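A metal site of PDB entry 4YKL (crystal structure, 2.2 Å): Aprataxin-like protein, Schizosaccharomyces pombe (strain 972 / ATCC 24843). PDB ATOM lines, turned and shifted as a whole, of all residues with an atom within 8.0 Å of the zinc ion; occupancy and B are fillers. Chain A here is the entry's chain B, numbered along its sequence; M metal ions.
The zinc ion is bound by OE1 of Glu 189 (2.0 Å), NE2 of His 185 (2.0 Å), SG of Cys 168 (2.3 Å) and SG of Cys 171 (2.3 Å).
The side-chain sulfur (SG) of Cys 168 sits close to the backbone NH (N) of Arg 170 (3.3 Å).
The side-chain carboxylate (OE2) of Glu 189 lies within salt-bridge range of the guanidinium group (NH1) of Arg 170, 2.9 Å away.
SG of Cys 171 lies close to N of Glu 173, 3.5 Å away.
The backbone NH (N) of Cys 168 is in hydrogen-bond range of the backbone carbonyl oxygen (O) of Glu 173 (2.8 Å).
Within 4 Å of the zinc ion: Cys 168, Cys 171, His 185 and Glu 189.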
ATOM      1  N   TYR A 134     -26.721 -11.836  19.735  1.00  0.00           N
ATOM      2  CA  TYR A 134     -25.476 -11.517  20.417  1.00  0.00           C
ATOM      3  C   TYR A 134     -24.979 -10.135  20.027  1.00  0.00           C
ATOM      4  O   TYR A 134     -24.685  -9.309  20.889  1.00  0.00           O
ATOM      5  CB  TYR A 134     -24.397 -12.568  20.118  1.00  0.00           C
ATOM      6  CG  TYR A 134     -23.095 -12.322  20.859  1.00  0.00           C
ATOM      7  CD1 TYR A 134     -23.026 -12.490  22.235  1.00  0.00           C
ATOM      8  CD2 TYR A 134     -21.951 -11.907  20.181  1.00  0.00           C
ATOM      9  CE1 TYR A 134     -21.834 -12.261  22.923  1.00  0.00           C
ATOM     10  CE2 TYR A 134     -20.761 -11.688  20.850  1.00  0.00           C
ATOM     11  CZ  TYR A 134     -20.703 -11.865  22.221  1.00  0.00           C
ATOM     12  OH  TYR A 134     -19.505 -11.639  22.880  1.00  0.00           O
ATOM     13  N   LYS A 167     -17.149 -11.745  18.362  1.00  0.00           N
ATOM     14  CA  LYS A 167     -16.036 -11.585  19.274  1.00  0.00           C
ATOM     15  C   LYS A 167     -16.509 -11.717  20.713  1.00  0.00           C
ATOM     16  O   LYS A 167     -17.611 -11.265  21.053  1.00  0.00           O
ATOM     17  CB  LYS A 167     -15.340 -10.237  19.081  1.00  0.00           C
ATOM     18  CG  LYS A 167     -14.795 -10.012  17.697  1.00  0.00           C
ATOM     19  CD  LYS A 167     -13.681  -8.975  17.720  1.00  0.00           C
ATOM     20  CE  LYS A 167     -13.268  -8.543  16.322  1.00  0.00           C
ATOM     21  NZ  LYS A 167     -12.891  -9.705  15.467  1.00  0.00           N
ATOM     22  N   CYS A 168     -15.685 -12.340  21.557  1.00  0.00           N
ATOM     23  CA  CYS A 168     -16.015 -12.426  22.961  1.00  0.00           C
ATOM     24  C   CYS A 168     -15.944 -11.037  23.566  1.00  0.00           C
ATOM     25  O   CYS A 168     -14.972 -10.305  23.370  1.00  0.00           O
ATOM     26  CB  CYS A 168     -15.087 -13.378  23.704  1.00  0.00           C
ATOM     27  SG  CYS A 168     -15.452 -13.447  25.464  1.00  0.00           S
ATOM     28  N   TRP A 169     -16.982 -10.682  24.306  1.00  0.00           N
ATOM     29  CA  TRP A 169     -17.101  -9.372  24.958  1.00  0.00           C
ATOM     30  C   TRP A 169     -16.119  -9.256  26.098  1.00  0.00           C
ATOM     31  O   TRP A 169     -15.824  -8.163  26.549  1.00  0.00           O
ATOM     32  CB  TRP A 169     -18.547  -9.148  25.496  1.00  0.00           C
ATOM     33  CG  TRP A 169     -18.932 -10.158  26.513  1.00  0.00           C
ATOM     34  CD1 TRP A 169     -19.591 -11.322  26.285  1.00  0.00           C
ATOM     35  CD2 TRP A 169     -18.621 -10.133  27.919  1.00  0.00           C
ATOM     36  NE1 TRP A 169     -19.731 -12.029  27.469  1.00  0.00           N
ATOM     37  CE2 TRP A 169     -19.147 -11.318  28.483  1.00  0.00           C
ATOM     38  CE3 TRP A 169     -17.951  -9.226  28.756  1.00  0.00           C
ATOM     39  CZ2 TRP A 169     -19.028 -11.619  29.846  1.00  0.00           C
ATOM     40  CZ3 TRP A 169     -17.834  -9.528  30.106  1.00  0.00           C
ATOM     41  CH2 TRP A 169     -18.367 -10.712  30.634  1.00  0.00           C
ATOM     42  N   ARG A 170     -15.616 -10.393  26.576  1.00  0.00           N
ATOM     43  CA  ARG A 170     -14.769 -10.377  27.772  1.00  0.00           C
ATOM     44  C   ARG A 170     -13.250 -10.448  27.505  1.00  0.00           C
ATOM     45  O   ARG A 170     -12.455  -9.921  28.287  1.00  0.00           O
ATOM     46  CB  ARG A 170     -15.188 -11.517  28.695  1.00  0.00           C
ATOM     47  CG  ARG A 170     -14.520 -11.472  30.059  1.00  0.00           C
ATOM     48  CD  ARG A 170     -15.200 -12.394  31.058  1.00  0.00           C
ATOM     49  NE  ARG A 170     -14.733 -12.158  32.412  1.00  0.00           N
ATOM     50  CZ  ARG A 170     -14.103 -13.055  33.164  1.00  0.00           C
ATOM     51  NH1 ARG A 170     -13.863 -14.274  32.683  1.00  0.00           N
ATOM     52  NH2 ARG A 170     -13.713 -12.748  34.398  1.00  0.00           N
ATOM     53  N   CYS A 171     -12.847 -11.084  26.409  1.00  0.00           N
ATOM     54  CA  CYS A 171     -11.424 -11.252  26.127  1.00  0.00           C
ATOM     55  C   CYS A 171     -11.094 -10.900  24.673  1.00  0.00           C
ATOM     56  O   CYS A 171      -9.929 -10.841  24.306  1.00  0.00           O
ATOM     57  CB  CYS A 171     -10.976 -12.696  26.416  1.00  0.00           C
ATOM     58  SG  CYS A 171     -11.529 -13.936  25.187  1.00  0.00           S
ATOM     59  N   GLY A 172     -12.112 -10.712  23.844  1.00  0.00           N
ATOM     60  CA  GLY A 172     -11.904 -10.320  22.476  1.00  0.00           C
ATOM     61  C   GLY A 172     -11.554 -11.429  21.487  1.00  0.00           C
ATOM     62  O   GLY A 172     -11.209 -11.140  20.342  1.00  0.00           O
ATOM     63  N   GLU A 173     -11.607 -12.687  21.923  1.00  0.00           N
ATOM     64  CA  GLU A 173     -11.371 -13.789  20.980  1.00  0.00           C
ATOM     65  C   GLU A 173     -12.431 -13.773  19.871  1.00  0.00           C
ATOM     66  O   GLU A 173     -13.628 -13.624  20.150  1.00  0.00           O
ATOM     67  CB  GLU A 173     -11.390 -15.146  21.690  1.00  0.00           C
ATOM     68  CG  GLU A 173     -10.871 -16.270  20.794  1.00  0.00           C
ATOM     69  CD  GLU A 173     -10.854 -17.658  21.459  1.00  0.00           C
ATOM     70  OE1 GLU A 173     -10.865 -17.735  22.705  1.00  0.00           O
ATOM     71  OE2 GLU A 173     -10.828 -18.665  20.717  1.00  0.00           O
ATOM     72  N   THR A 174     -11.980 -13.927  18.638  1.00  0.00           N
ATOM     73  CA  THR A 174     -12.869 -13.970  17.482  1.00  0.00           C
ATOM     74  C   THR A 174     -13.298 -15.393  17.153  1.00  0.00           C
ATOM     75  O   THR A 174     -12.533 -16.342  17.342  1.00  0.00           O
ATOM     76  CB  THR A 174     -12.205 -13.360  16.216  1.00  0.00           C
ATOM     77  OG1 THR A 174     -13.068 -13.549  15.082  1.00  0.00           O
ATOM     78  CG2 THR A 174     -10.891 -14.041  15.932  1.00  0.00           C
ATOM     79  N   PHE A 175     -14.527 -15.531  16.660  1.00  0.00           N
ATOM     80  CA  PHE A 175     -15.075 -16.844  16.342  1.00  0.00           C
ATOM     81  C   PHE A 175     -15.621 -16.881  14.929  1.00  0.00           C
ATOM     82  O   PHE A 175     -16.273 -17.841  14.537  1.00  0.00           O
ATOM     83  CB  PHE A 175     -16.157 -17.219  17.359  1.00  0.00           C
ATOM     84  CG  PHE A 175     -15.624 -17.430  18.748  1.00  0.00           C
ATOM     85  CD1 PHE A 175     -15.174 -18.673  19.155  1.00  0.00           C
ATOM     86  CD2 PHE A 175     -15.518 -16.369  19.644  1.00  0.00           C
ATOM     87  CE1 PHE A 175     -14.652 -18.869  20.429  1.00  0.00           C
ATOM     88  CE2 PHE A 175     -15.017 -16.553  20.919  1.00  0.00           C
ATOM     89  CZ  PHE A 175     -14.579 -17.807  21.308  1.00  0.00           C
ATOM     90  N   LEU A 182     -18.873 -19.760  19.774  1.00  0.00           N
ATOM     91  CA  LEU A 182     -19.033 -18.631  20.694  1.00  0.00           C
ATOM     92  C   LEU A 182     -19.841 -19.038  21.933  1.00  0.00           C
ATOM     93  O   LEU A 182     -19.417 -18.747  23.056  1.00  0.00           O
ATOM     94  CB  LEU A 182     -19.697 -17.443  20.010  1.00  0.00           C
ATOM     95  CG  LEU A 182     -20.014 -16.259  20.933  1.00  0.00           C
ATOM     96  CD1 LEU A 182     -18.711 -15.508  21.397  1.00  0.00           C
ATOM     97  CD2 LEU A 182     -21.033 -15.293  20.325  1.00  0.00           C
ATOM     98  N   HIS A 185     -17.860 -20.902  24.388  1.00  0.00           N
ATOM     99  CA  HIS A 185     -16.892 -20.013  25.052  1.00  0.00           C
ATOM    100  C   HIS A 185     -17.555 -19.097  26.078  1.00  0.00           C
ATOM    101  O   HIS A 185     -16.986 -18.827  27.138  1.00  0.00           O
ATOM    102  CB  HIS A 185     -16.152 -19.185  23.991  1.00  0.00           C
ATOM    103  CG  HIS A 185     -15.111 -18.255  24.566  1.00  0.00           C
ATOM    104  ND1 HIS A 185     -13.840 -18.676  24.896  1.00  0.00           N
ATOM    105  CD2 HIS A 185     -15.162 -16.927  24.830  1.00  0.00           C
ATOM    106  CE1 HIS A 185     -13.152 -17.640  25.353  1.00  0.00           C
ATOM    107  NE2 HIS A 185     -13.922 -16.573  25.321  1.00  0.00           N
ATOM    108  N   LEU A 186     -18.772 -18.615  25.797  1.00  0.00           N
ATOM    109  CA  LEU A 186     -19.463 -17.754  26.748  1.00  0.00           C
ATOM    110  C   LEU A 186     -19.761 -18.506  28.062  1.00  0.00           C
ATOM    111  O   LEU A 186     -19.703 -17.913  29.158  1.00  0.00           O
ATOM    112  CB  LEU A 186     -20.750 -17.210  26.144  1.00  0.00           C
ATOM    113  CG  LEU A 186     -20.582 -16.266  24.946  1.00  0.00           C
ATOM    114  CD1 LEU A 186     -21.956 -15.835  24.428  1.00  0.00           C
ATOM    115  CD2 LEU A 186     -19.732 -15.052  25.310  1.00  0.00           C
ATOM    116  N   GLU A 188     -17.873 -20.994  29.251  1.00  0.00           N
ATOM    117  CA  GLU A 188     -16.564 -21.015  29.898  1.00  0.00           C
ATOM    118  C   GLU A 188     -16.185 -19.681  30.556  1.00  0.00           C
ATOM    119  O   GLU A 188     -15.734 -19.657  31.696  1.00  0.00           O
ATOM    120  CB  GLU A 188     -15.484 -21.411  28.897  1.00  0.00           C
ATOM    121  CG  GLU A 188     -15.686 -22.775  28.251  1.00  0.00           C
ATOM    122  CD  GLU A 188     -14.815 -22.970  27.018  1.00  0.00           C
ATOM    123  OE1 GLU A 188     -15.190 -23.805  26.155  1.00  0.00           O
ATOM    124  OE2 GLU A 188     -13.763 -22.292  26.903  1.00  0.00           O
ATOM    125  N   GLU A 189     -16.350 -18.573  29.835  1.00  0.00           N
ATOM    126  CA  GLU A 189     -16.111 -17.261  30.432  1.00  0.00           C
ATOM    127  C   GLU A 189     -16.957 -17.067  31.698  1.00  0.00           C
ATOM    128  O   GLU A 189     -16.486 -16.507  32.684  1.00  0.00           O
ATOM    129  CB  GLU A 189     -16.394 -16.126  29.437  1.00  0.00           C
ATOM    130  CG  GLU A 189     -15.359 -15.989  28.321  1.00  0.00           C
ATOM    131  CD  GLU A 189     -14.018 -15.372  28.762  1.00  0.00           C
ATOM    132  OE1 GLU A 189     -13.241 -14.985  27.877  1.00  0.00           O
ATOM    133  OE2 GLU A 189     -13.744 -15.265  29.983  1.00  0.00           O
ATOM    134  N   TYR A 190     -18.192 -17.546  31.662  1.00  0.00           N
ATOM    135  CA  TYR A 190     -19.090 -17.359  32.793  1.00  0.00           C
ATOM    136  C   TYR A 190     -18.685 -18.213  33.992  1.00  0.00           C
ATOM    137  O   TYR A 190     -18.675 -17.708  35.121  1.00  0.00           O
ATOM    138  CB  TYR A 190     -20.540 -17.672  32.408  1.00  0.00           C
ATOM    139  CG  TYR A 190     -21.453 -17.643  33.612  1.00  0.00           C
ATOM    140  CD1 TYR A 190     -21.876 -16.436  34.151  1.00  0.00           C
ATOM    141  CD2 TYR A 190     -21.859 -18.832  34.222  1.00  0.00           C
ATOM    142  CE1 TYR A 190     -22.691 -16.407  35.268  1.00  0.00           C
ATOM    143  CE2 TYR A 190     -22.675 -18.810  35.333  1.00  0.00           C
ATOM    144  CZ  TYR A 190     -23.093 -17.585  35.847  1.00  0.00           C
ATOM    145  OH  TYR A 190     -23.910 -17.557  36.950  1.00  0.00           O
HETATM  146 ZN    ZN M   1     -13.571 -14.699  25.970  1.00  0.00          ZN
